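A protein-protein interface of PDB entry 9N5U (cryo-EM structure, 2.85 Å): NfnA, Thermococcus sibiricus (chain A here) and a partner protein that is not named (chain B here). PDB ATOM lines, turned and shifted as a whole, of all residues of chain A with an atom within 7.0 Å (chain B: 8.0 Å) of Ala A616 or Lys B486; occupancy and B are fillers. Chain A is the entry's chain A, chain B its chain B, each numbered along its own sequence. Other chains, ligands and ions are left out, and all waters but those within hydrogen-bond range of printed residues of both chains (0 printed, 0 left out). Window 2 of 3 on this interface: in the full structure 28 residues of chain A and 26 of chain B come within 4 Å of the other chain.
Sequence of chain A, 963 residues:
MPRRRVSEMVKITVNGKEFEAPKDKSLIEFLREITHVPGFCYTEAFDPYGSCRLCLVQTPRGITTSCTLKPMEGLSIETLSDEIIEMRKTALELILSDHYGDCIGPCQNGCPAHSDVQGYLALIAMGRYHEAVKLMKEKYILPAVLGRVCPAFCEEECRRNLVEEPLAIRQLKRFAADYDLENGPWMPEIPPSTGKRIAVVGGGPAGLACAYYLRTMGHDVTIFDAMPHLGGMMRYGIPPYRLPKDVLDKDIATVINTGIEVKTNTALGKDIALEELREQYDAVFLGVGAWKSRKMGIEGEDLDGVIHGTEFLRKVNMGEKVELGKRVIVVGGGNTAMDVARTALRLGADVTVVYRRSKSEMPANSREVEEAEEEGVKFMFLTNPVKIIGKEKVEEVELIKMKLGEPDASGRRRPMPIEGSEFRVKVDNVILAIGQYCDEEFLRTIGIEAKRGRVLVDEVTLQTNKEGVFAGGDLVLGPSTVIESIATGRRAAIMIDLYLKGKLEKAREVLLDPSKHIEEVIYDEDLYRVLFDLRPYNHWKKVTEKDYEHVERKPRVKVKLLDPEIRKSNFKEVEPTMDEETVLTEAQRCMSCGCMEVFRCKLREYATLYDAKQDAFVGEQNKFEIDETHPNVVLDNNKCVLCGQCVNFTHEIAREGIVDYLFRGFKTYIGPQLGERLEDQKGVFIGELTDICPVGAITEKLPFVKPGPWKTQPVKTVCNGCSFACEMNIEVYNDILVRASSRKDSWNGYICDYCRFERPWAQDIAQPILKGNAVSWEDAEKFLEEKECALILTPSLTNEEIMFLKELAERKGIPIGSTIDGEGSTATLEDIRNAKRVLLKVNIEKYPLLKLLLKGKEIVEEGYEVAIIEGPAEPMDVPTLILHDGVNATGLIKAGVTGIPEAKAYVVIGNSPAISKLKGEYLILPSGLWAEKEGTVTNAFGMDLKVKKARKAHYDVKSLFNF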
ATOM      1  N   LYS A  89     -15.561 -25.395  20.583  1.00  0.00           N
ATOM      2  CA  LYS A  89     -15.056 -24.763  19.373  1.00  0.00           C
ATOM      3  C   LYS A  89     -16.123 -23.898  18.718  1.00  0.00           C
ATOM      4  O   LYS A  89     -15.849 -22.768  18.302  1.00  0.00           O
ATOM      5  CB  LYS A  89     -14.568 -25.849  18.416  1.00  0.00           C
ATOM      6  CG  LYS A  89     -13.563 -25.419  17.382  1.00  0.00           C
ATOM      7  CD  LYS A  89     -12.994 -26.645  16.689  1.00  0.00           C
ATOM      8  CE  LYS A  89     -12.116 -26.272  15.521  1.00  0.00           C
ATOM      9  NZ  LYS A  89     -11.581 -27.477  14.847  1.00  0.00           N
ATOM     10  N   GLU A  93     -16.085 -19.861  18.253  1.00  0.00           N
ATOM     11  CA  GLU A  93     -16.273 -19.259  16.937  1.00  0.00           C
ATOM     12  C   GLU A  93     -17.451 -18.291  16.931  1.00  0.00           C
ATOM     13  O   GLU A  93     -17.401 -17.244  16.272  1.00  0.00           O
ATOM     14  CB  GLU A  93     -16.451 -20.354  15.890  1.00  0.00           C
ATOM     15  CG  GLU A  93     -15.179 -21.137  15.634  1.00  0.00           C
ATOM     16  CD  GLU A  93     -15.415 -22.420  14.875  1.00  0.00           C
ATOM     17  OE1 GLU A  93     -16.581 -22.723  14.562  1.00  0.00           O
ATOM     18  OE2 GLU A  93     -14.432 -23.127  14.589  1.00  0.00           O
ATOM     19  N   LEU A  94     -18.509 -18.611  17.679  1.00  0.00           N
ATOM     20  CA  LEU A  94     -19.629 -17.691  17.836  1.00  0.00           C
ATOM     21  C   LEU A  94     -19.197 -16.406  18.526  1.00  0.00           C
ATOM     22  O   LEU A  94     -19.618 -15.311  18.136  1.00  0.00           O
ATOM     23  CB  LEU A  94     -20.748 -18.359  18.629  1.00  0.00           C
ATOM     24  CG  LEU A  94     -21.609 -19.423  17.954  1.00  0.00           C
ATOM     25  CD1 LEU A  94     -22.507 -20.075  18.985  1.00  0.00           C
ATOM     26  CD2 LEU A  94     -22.433 -18.818  16.843  1.00  0.00           C
ATOM     27  N   SER A  97     -17.120 -14.323  16.172  1.00  0.00           N
ATOM     28  CA  SER A  97     -17.921 -13.705  15.124  1.00  0.00           C
ATOM     29  C   SER A  97     -18.463 -12.337  15.522  1.00  0.00           C
ATOM     30  O   SER A  97     -18.846 -11.561  14.643  1.00  0.00           O
ATOM     31  CB  SER A  97     -19.073 -14.628  14.738  1.00  0.00           C
ATOM     32  OG  SER A  97     -19.923 -14.873  15.840  1.00  0.00           O
ATOM     33  N   ALA A 612      -9.749 -22.229  16.746  1.00  0.00           N
ATOM     34  CA  ALA A 612     -10.918 -21.463  16.352  1.00  0.00           C
ATOM     35  C   ALA A 612     -10.585 -20.528  15.199  1.00  0.00           C
ATOM     36  O   ALA A 612      -9.553 -19.854  15.201  1.00  0.00           O
ATOM     37  CB  ALA A 612     -11.461 -20.668  17.536  1.00  0.00           C
ATOM     38  N   LYS A 613     -11.465 -20.502  14.207  1.00  0.00           N
ATOM     39  CA  LYS A 613     -11.316 -19.634  13.053  1.00  0.00           C
ATOM     40  C   LYS A 613     -12.215 -18.419  13.218  1.00  0.00           C
ATOM     41  O   LYS A 613     -13.309 -18.516  13.778  1.00  0.00           O
ATOM     42  CB  LYS A 613     -11.663 -20.367  11.756  1.00  0.00           C
ATOM     43  CG  LYS A 613     -10.846 -21.620  11.499  1.00  0.00           C
ATOM     44  CD  LYS A 613      -9.366 -21.310  11.414  1.00  0.00           C
ATOM     45  CE  LYS A 613      -8.545 -22.579  11.332  1.00  0.00           C
ATOM     46  NZ  LYS A 613      -7.098 -22.312  11.518  1.00  0.00           N
ATOM     47  N   GLN A 614     -11.736 -17.272  12.742  1.00  0.00           N
ATOM     48  CA  GLN A 614     -12.520 -16.046  12.811  1.00  0.00           C
ATOM     49  C   GLN A 614     -13.634 -16.025  11.772  1.00  0.00           C
ATOM     50  O   GLN A 614     -14.665 -15.381  11.988  1.00  0.00           O
ATOM     51  CB  GLN A 614     -11.601 -14.840  12.633  1.00  0.00           C
ATOM     52  CG  GLN A 614     -12.273 -13.497  12.796  1.00  0.00           C
ATOM     53  CD  GLN A 614     -11.320 -12.354  12.569  1.00  0.00           C
ATOM     54  OE1 GLN A 614     -10.113 -12.500  12.735  1.00  0.00           O
ATOM     55  NE2 GLN A 614     -11.854 -11.208  12.181  1.00  0.00           N
ATOM     56  N   ASP A 615     -13.455 -16.727  10.658  1.00  0.00           N
ATOM     57  CA  ASP A 615     -14.408 -16.713   9.559  1.00  0.00           C
ATOM     58  C   ASP A 615     -15.339 -17.916   9.568  1.00  0.00           C
ATOM     59  O   ASP A 615     -16.011 -18.170   8.564  1.00  0.00           O
ATOM     60  CB  ASP A 615     -13.667 -16.640   8.223  1.00  0.00           C
ATOM     61  CG  ASP A 615     -12.613 -17.710   8.087  1.00  0.00           C
ATOM     62  OD1 ASP A 615     -11.930 -18.001   9.089  1.00  0.00           O
ATOM     63  OD2 ASP A 615     -12.465 -18.264   6.979  1.00  0.00           O
ATOM     64  N   ALA A 616     -15.383 -18.669  10.668  1.00  0.00           N
ATOM     65  CA  ALA A 616     -16.285 -19.813  10.755  1.00  0.00           C
ATOM     66  C   ALA A 616     -17.740 -19.367  10.705  1.00  0.00           C
ATOM     67  O   ALA A 616     -18.567 -19.978  10.021  1.00  0.00           O
ATOM     68  CB  ALA A 616     -16.005 -20.601  12.029  1.00  0.00           C
ATOM     69  N   PHE A 617     -18.072 -18.307  11.431  1.00  0.00           N
ATOM     70  CA  PHE A 617     -19.368 -17.652  11.336  1.00  0.00           C
ATOM     71  C   PHE A 617     -19.117 -16.187  11.023  1.00  0.00           C
ATOM     72  O   PHE A 617     -18.394 -15.506  11.755  1.00  0.00           O
ATOM     73  CB  PHE A 617     -20.173 -17.813  12.627  1.00  0.00           C
ATOM     74  CG  PHE A 617     -20.470 -19.241  12.974  1.00  0.00           C
ATOM     75  CD1 PHE A 617     -21.460 -19.935  12.304  1.00  0.00           C
ATOM     76  CD2 PHE A 617     -19.755 -19.893  13.963  1.00  0.00           C
ATOM     77  CE1 PHE A 617     -21.732 -21.249  12.612  1.00  0.00           C
ATOM     78  CE2 PHE A 617     -20.023 -21.208  14.275  1.00  0.00           C
ATOM     79  CZ  PHE A 617     -21.013 -21.886  13.598  1.00  0.00           C
ATOM     80  N   VAL A 618     -19.683 -15.713   9.921  1.00  0.00           N
ATOM     81  CA  VAL A 618     -19.513 -14.337   9.481  1.00  0.00           C
ATOM     82  C   VAL A 618     -20.895 -13.728   9.328  1.00  0.00           C
ATOM     83  O   VAL A 618     -21.789 -14.343   8.736  1.00  0.00           O
ATOM     84  CB  VAL A 618     -18.722 -14.246   8.163  1.00  0.00           C
ATOM     85  CG1 VAL A 618     -18.430 -12.800   7.823  1.00  0.00           C
ATOM     86  CG2 VAL A 618     -17.433 -15.027   8.259  1.00  0.00           C
ATOM     87  N   ARG B 466     -26.919 -16.169  14.263  1.00  0.00           N
ATOM     88  CA  ARG B 466     -26.246 -16.806  13.132  1.00  0.00           C
ATOM     89  C   ARG B 466     -27.191 -17.720  12.353  1.00  0.00           C
ATOM     90  O   ARG B 466     -27.157 -17.748  11.117  1.00  0.00           O
ATOM     91  CB  ARG B 466     -25.018 -17.572  13.614  1.00  0.00           C
ATOM     92  CG  ARG B 466     -23.954 -16.694  14.251  1.00  0.00           C
ATOM     93  CD  ARG B 466     -23.696 -15.442  13.435  1.00  0.00           C
ATOM     94  NE  ARG B 466     -22.831 -14.504  14.135  1.00  0.00           N
ATOM     95  CZ  ARG B 466     -22.815 -13.197  13.913  1.00  0.00           C
ATOM     96  NH1 ARG B 466     -23.615 -12.638  13.022  1.00  0.00           N
ATOM     97  NH2 ARG B 466     -21.983 -12.431  14.609  1.00  0.00           N
ATOM     98  N   MET B 467     -28.054 -18.460  13.055  1.00  0.00           N
ATOM     99  CA  MET B 467     -29.046 -19.291  12.382  1.00  0.00           C
ATOM    100  C   MET B 467     -30.048 -18.446  11.605  1.00  0.00           C
ATOM    101  O   MET B 467     -30.424 -18.798  10.480  1.00  0.00           O
ATOM    102  CB  MET B 467     -29.768 -20.179  13.395  1.00  0.00           C
ATOM    103  CG  MET B 467     -28.946 -21.357  13.878  1.00  0.00           C
ATOM    104  SD  MET B 467     -29.930 -22.654  14.641  1.00  0.00           S
ATOM    105  CE  MET B 467     -30.359 -21.888  16.193  1.00  0.00           C
ATOM    106  N   LEU B 470     -28.363 -17.233   8.476  1.00  0.00           N
ATOM    107  CA  LEU B 470     -28.314 -18.297   7.476  1.00  0.00           C
ATOM    108  C   LEU B 470     -29.671 -18.491   6.808  1.00  0.00           C
ATOM    109  O   LEU B 470     -29.750 -18.685   5.589  1.00  0.00           O
ATOM    110  CB  LEU B 470     -27.833 -19.597   8.115  1.00  0.00           C
ATOM    111  CG  LEU B 470     -26.359 -19.601   8.517  1.00  0.00           C
ATOM    112  CD1 LEU B 470     -26.026 -20.802   9.379  1.00  0.00           C
ATOM    113  CD2 LEU B 470     -25.481 -19.574   7.284  1.00  0.00           C
ATOM    114  N   LYS B 473     -30.217 -15.698   4.428  1.00  0.00           N
ATOM    115  CA  LYS B 473     -29.383 -15.927   3.254  1.00  0.00           C
ATOM    116  C   LYS B 473     -30.023 -16.937   2.309  1.00  0.00           C
ATOM    117  O   LYS B 473     -30.016 -16.746   1.088  1.00  0.00           O
ATOM    118  CB  LYS B 473     -28.001 -16.406   3.693  1.00  0.00           C
ATOM    119  CG  LYS B 473     -26.933 -16.317   2.630  1.00  0.00           C
ATOM    120  CD  LYS B 473     -25.677 -17.054   3.059  1.00  0.00           C
ATOM    121  CE  LYS B 473     -25.209 -16.611   4.428  1.00  0.00           C
ATOM    122  NZ  LYS B 473     -24.868 -15.165   4.456  1.00  0.00           N
ATOM    123  N   ILE B 474     -30.572 -18.022   2.859  1.00  0.00           N
ATOM    124  CA  ILE B 474     -31.226 -19.035   2.033  1.00  0.00           C
ATOM    125  C   ILE B 474     -32.491 -18.473   1.394  1.00  0.00           C
ATOM    126  O   ILE B 474     -32.791 -18.753   0.227  1.00  0.00           O
ATOM    127  CB  ILE B 474     -31.522 -20.292   2.873  1.00  0.00           C
ATOM    128  CG1 ILE B 474     -30.224 -20.935   3.351  1.00  0.00           C
ATOM    129  CG2 ILE B 474     -32.328 -21.299   2.077  1.00  0.00           C
ATOM    130  CD1 ILE B 474     -30.432 -22.136   4.231  1.00  0.00           C
ATOM    131  N   ALA B 480     -26.293 -21.609  -0.408  1.00  0.00           N
ATOM    132  CA  ALA B 480     -25.663 -22.760  -1.030  1.00  0.00           C
ATOM    133  C   ALA B 480     -25.864 -23.952  -0.107  1.00  0.00           C
ATOM    134  O   ALA B 480     -26.523 -23.850   0.931  1.00  0.00           O
ATOM    135  CB  ALA B 480     -24.180 -22.504  -1.308  1.00  0.00           C
ATOM    136  N   LEU B 481     -25.292 -25.091  -0.492  1.00  0.00           N
ATOM    137  CA  LEU B 481     -25.372 -26.273   0.358  1.00  0.00           C
ATOM    138  C   LEU B 481     -24.578 -26.097   1.645  1.00  0.00           C
ATOM    139  O   LEU B 481     -24.921 -26.698   2.673  1.00  0.00           O
ATOM    140  CB  LEU B 481     -24.881 -27.500  -0.404  1.00  0.00           C
ATOM    141  CG  LEU B 481     -25.832 -28.047  -1.462  1.00  0.00           C
ATOM    142  CD1 LEU B 481     -25.197 -29.216  -2.183  1.00  0.00           C
ATOM    143  CD2 LEU B 481     -27.129 -28.465  -0.811  1.00  0.00           C
ATOM    144  N   GLU B 482     -23.521 -25.285   1.611  1.00  0.00           N
ATOM    145  CA  GLU B 482     -22.741 -25.048   2.818  1.00  0.00           C
ATOM    146  C   GLU B 482     -23.554 -24.314   3.875  1.00  0.00           C
ATOM    147  O   GLU B 482     -23.332 -24.520   5.069  1.00  0.00           O
ATOM    148  CB  GLU B 482     -21.467 -24.278   2.480  1.00  0.00           C
ATOM    149  CG  GLU B 482     -21.692 -23.009   1.697  1.00  0.00           C
ATOM    150  CD  GLU B 482     -20.395 -22.369   1.257  1.00  0.00           C
ATOM    151  OE1 GLU B 482     -19.331 -22.989   1.461  1.00  0.00           O
ATOM    152  OE2 GLU B 482     -20.436 -21.249   0.709  1.00  0.00           O
ATOM    153  N   ASP B 483     -24.506 -23.475   3.462  1.00  0.00           N
ATOM    154  CA  ASP B 483     -25.389 -22.826   4.426  1.00  0.00           C
ATOM    155  C   ASP B 483     -26.290 -23.837   5.123  1.00  0.00           C
ATOM    156  O   ASP B 483     -26.489 -23.765   6.341  1.00  0.00           O
ATOM    157  CB  ASP B 483     -26.222 -21.754   3.731  1.00  0.00           C
ATOM    158  CG  ASP B 483     -25.389 -20.578   3.288  1.00  0.00           C
ATOM    159  OD1 ASP B 483     -24.561 -20.101   4.087  1.00  0.00           O
ATOM    160  OD2 ASP B 483     -25.549 -20.137   2.138  1.00  0.00           O
ATOM    161  N   ILE B 484     -26.839 -24.789   4.367  1.00  0.00           N
ATOM    162  CA  ILE B 484     -27.679 -25.823   4.963  1.00  0.00           C
ATOM    163  C   ILE B 484     -26.863 -26.687   5.915  1.00  0.00           C
ATOM    164  O   ILE B 484     -27.332 -27.054   6.999  1.00  0.00           O
ATOM    165  CB  ILE B 484     -28.354 -26.660   3.860  1.00  0.00           C
ATOM    166  CG1 ILE B 484     -29.431 -25.835   3.160  1.00  0.00           C
ATOM    167  CG2 ILE B 484     -28.949 -27.936   4.424  1.00  0.00           C
ATOM    168  CD1 ILE B 484     -30.251 -26.625   2.184  1.00  0.00           C
ATOM    169  N   GLU B 485     -25.629 -27.016   5.532  1.00  0.00           N
ATOM    170  CA  GLU B 485     -24.778 -27.813   6.411  1.00  0.00           C
ATOM    171  C   GLU B 485     -24.388 -27.038   7.667  1.00  0.00           C
ATOM    172  O   GLU B 485     -24.301 -27.615   8.758  1.00  0.00           O
ATOM    173  CB  GLU B 485     -23.546 -28.281   5.648  1.00  0.00           C
ATOM    174  CG  GLU B 485     -23.886 -29.180   4.478  1.00  0.00           C
ATOM    175  CD  GLU B 485     -22.750 -29.308   3.493  1.00  0.00           C
ATOM    176  OE1 GLU B 485     -21.693 -28.685   3.721  1.00  0.00           O
ATOM    177  OE2 GLU B 485     -22.913 -30.029   2.488  1.00  0.00           O
ATOM    178  N   LYS B 486     -24.163 -25.728   7.537  1.00  0.00           N
ATOM    179  CA  LYS B 486     -23.924 -24.893   8.709  1.00  0.00           C
ATOM    180  C   LYS B 486     -25.132 -24.878   9.634  1.00  0.00           C
ATOM    181  O   LYS B 486     -24.981 -24.930  10.857  1.00  0.00           O
ATOM    182  CB  LYS B 486     -23.571 -23.471   8.283  1.00  0.00           C
ATOM    183  CG  LYS B 486     -22.092 -23.163   8.276  1.00  0.00           C
ATOM    184  CD  LYS B 486     -21.865 -21.705   7.953  1.00  0.00           C
ATOM    185  CE  LYS B 486     -20.398 -21.388   7.826  1.00  0.00           C
ATOM    186  NZ  LYS B 486     -20.187 -19.938   7.592  1.00  0.00           N
ATOM    187  N   LEU B 487     -26.338 -24.795   9.069  1.00  0.00           N
ATOM    188  CA  LEU B 487     -27.542 -24.859   9.891  1.00  0.00           C
ATOM    189  C   LEU B 487     -27.643 -26.197  10.613  1.00  0.00           C
ATOM    190  O   LEU B 487     -27.932 -26.251  11.815  1.00  0.00           O
ATOM    191  CB  LEU B 487     -28.783 -24.628   9.029  1.00  0.00           C
ATOM    192  CG  LEU B 487     -29.242 -23.189   8.827  1.00  0.00           C
ATOM    193  CD1 LEU B 487     -30.506 -23.165   7.997  1.00  0.00           C
ATOM    194  CD2 LEU B 487     -29.467 -22.522  10.165  1.00  0.00           C
ATOM    195  N   GLU B 488     -27.399 -27.291   9.887  1.00  0.00           N
ATOM    196  CA  GLU B 488     -27.519 -28.624  10.466  1.00  0.00           C
ATOM    197  C   GLU B 488     -26.473 -28.874  11.537  1.00  0.00           C
ATOM    198  O   GLU B 488     -26.692 -29.696  12.430  1.00  0.00           O
ATOM    199  CB  GLU B 488     -27.406 -29.688   9.377  1.00  0.00           C
ATOM    200  CG  GLU B 488     -28.637 -29.829   8.516  1.00  0.00           C
ATOM    201  CD  GLU B 488     -28.506 -30.934   7.495  1.00  0.00           C
ATOM    202  OE1 GLU B 488     -27.380 -31.175   7.018  1.00  0.00           O
ATOM    203  OE2 GLU B 488     -29.527 -31.570   7.176  1.00  0.00           O
ATOM    204  N   LYS B 489     -25.326 -28.204  11.451  1.00  0.00           N
ATOM    205  CA  LYS B 489     -24.321 -28.347  12.494  1.00  0.00           C
ATOM    206  C   LYS B 489     -24.617 -27.440  13.684  1.00  0.00           C
ATOM    207  O   LYS B 489     -24.478 -27.858  14.838  1.00  0.00           O
ATOM    208  CB  LYS B 489     -22.937 -28.046  11.923  1.00  0.00           C
ATOM    209  CG  LYS B 489     -21.815 -28.107  12.932  1.00  0.00           C
ATOM    210  CD  LYS B 489     -20.626 -27.303  12.457  1.00  0.00           C
ATOM    211  CE  LYS B 489     -20.997 -25.842  12.286  1.00  0.00           C
ATOM    212  NZ  LYS B 489     -19.854 -25.040  11.784  1.00  0.00           N
ATOM    213  N   LEU B 490     -25.054 -26.209  13.418  1.00  0.00           N
ATOM    214  CA  LEU B 490     -25.213 -25.203  14.458  1.00  0.00           C
ATOM    215  C   LEU B 490     -26.447 -25.445  15.321  1.00  0.00           C
ATOM    216  O   LEU B 490     -26.396 -25.238  16.536  1.00  0.00           O
ATOM    217  CB  LEU B 490     -25.268 -23.817  13.814  1.00  0.00           C
ATOM    218  CG  LEU B 490     -25.285 -22.575  14.704  1.00  0.00           C
ATOM    219  CD1 LEU B 490     -24.109 -22.568  15.657  1.00  0.00           C
ATOM    220  CD2 LEU B 490     -25.271 -21.336  13.837  1.00  0.00           C
ATOM    221  N   ALA B 491     -27.560 -25.875  14.720  1.00  0.00           N
ATOM    222  CA  ALA B 491     -28.808 -26.009  15.473  1.00  0.00           C
ATOM    223  C   ALA B 491     -28.739 -27.012  16.628  1.00  0.00           C
ATOM    224  O   ALA B 491     -29.197 -26.671  17.735  1.00  0.00           O
ATOM    225  CB  ALA B 491     -29.948 -26.335  14.503  1.00  0.00           C
ATOM    226  N   PRO B 492     -28.209 -28.234  16.463  1.00  0.00           N
ATOM    227  CA  PRO B 492     -28.074 -29.118  17.633  1.00  0.00           C
ATOM    228  C   PRO B 492     -27.194 -28.542  18.723  1.00  0.00           C
ATOM    229  O   PRO B 492     -27.443 -28.791  19.908  1.00  0.00           O
ATOM    230  CB  PRO B 492     -27.462 -30.394  17.040  1.00  0.00           C
ATOM    231  CG  PRO B 492     -27.805 -30.357  15.617  1.00  0.00           C
ATOM    232  CD  PRO B 492     -27.773 -28.921  15.236  1.00  0.00           C
ATOM    233  N   LEU B 493     -26.175 -27.768  18.362  1.00  0.00           N
ATOM    234  CA  LEU B 493     -25.296 -27.192  19.370  1.00  0.00           C
ATOM    235  C   LEU B 493     -25.974 -26.053  20.120  1.00  0.00           C
ATOM    236  O   LEU B 493     -25.763 -25.894  21.326  1.00  0.00           O
ATOM    237  CB  LEU B 493     -23.997 -26.724  18.719  1.00  0.00           C
ATOM    238  CG  LEU B 493     -23.285 -27.815  17.920  1.00  0.00           C
ATOM    239  CD1 LEU B 493     -22.121 -27.244  17.153  1.00  0.00           C
ATOM    240  CD2 LEU B 493     -22.826 -28.938  18.825  1.00  0.00           C
ATOM    241  N   VAL B 510     -36.183 -24.951  13.095  1.00  0.00           N
ATOM    242  CA  VAL B 510     -35.210 -25.207  12.035  1.00  0.00           C
ATOM    243  C   VAL B 510     -34.952 -26.699  11.904  1.00  0.00           C
ATOM    244  O   VAL B 510     -34.934 -27.253  10.799  1.00  0.00           O
ATOM    245  CB  VAL B 510     -33.908 -24.432  12.307  1.00  0.00           C
ATOM    246  CG1 VAL B 510     -32.776 -24.967  11.456  1.00  0.00           C
ATOM    247  CG2 VAL B 510     -34.114 -22.968  12.040  1.00  0.00           C
ATOM    248  N   LEU B 514     -35.945 -28.889   8.596  1.00  0.00           N
ATOM    249  CA  LEU B 514     -34.917 -29.633   7.876  1.00  0.00           C
ATOM    250  C   LEU B 514     -35.230 -31.123   7.846  1.00  0.00           C
ATOM    251  O   LEU B 514     -34.958 -31.800   6.849  1.00  0.00           O
ATOM    252  CB  LEU B 514     -33.549 -29.395   8.512  1.00  0.00           C
ATOM    253  CG  LEU B 514     -32.850 -28.070   8.234  1.00  0.00           C
ATOM    254  CD1 LEU B 514     -31.682 -27.898   9.177  1.00  0.00           C
ATOM    255  CD2 LEU B 514     -32.382 -28.016   6.799  1.00  0.00           C
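O of Ser A97 sits at hydrogen-bond distance from NH2 of Arg B466 (3.3 Å). O of Ala A616 lies within hydrogen-bond range of NZ of Lys B486 (2.9 Å).
Hydrophobic or aromatic side chains of chain A that line the printed part of chain B: Leu A94 and Phe A617. Among the printed residues, no Asp or Glu carboxylate lies within 4 Å of a Lys or Arg side-chain nitrogen of the other chain.
Of the printed residues of chain B, Leu A94 touches Arg B466 (3.7 Å). Of chain B, only Lys B486 (2.9 Å) comes within 4 Å of Ala A616. Of the printed residues of chain B, Phe A617 touches Lys B489 (3.8 Å) and Leu B490 (3.7 Å). Of the printed residues of chain A, Lys B489 touches Phe A617 (3.8 Å). Of the printed residues of chain A, Leu B490 touches Phe A617. The nearest residue of chain B that does not touch Ala A616 is Lys B489 (5.5 Å). The nearest residue of chain A that does not touch Lys B486 is Phe A617 (4.5 Å).
Leu A94 touches Arg B466. CZ of Phe A617 touches NZ of Lys B489 (3.8 Å). Phe A617 touches Leu B490.
The side-chain hydroxyl (OG) of Ser A97 sits close to the backbone carbonyl oxygen (O) of Glu A93, 3.5 Å away.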
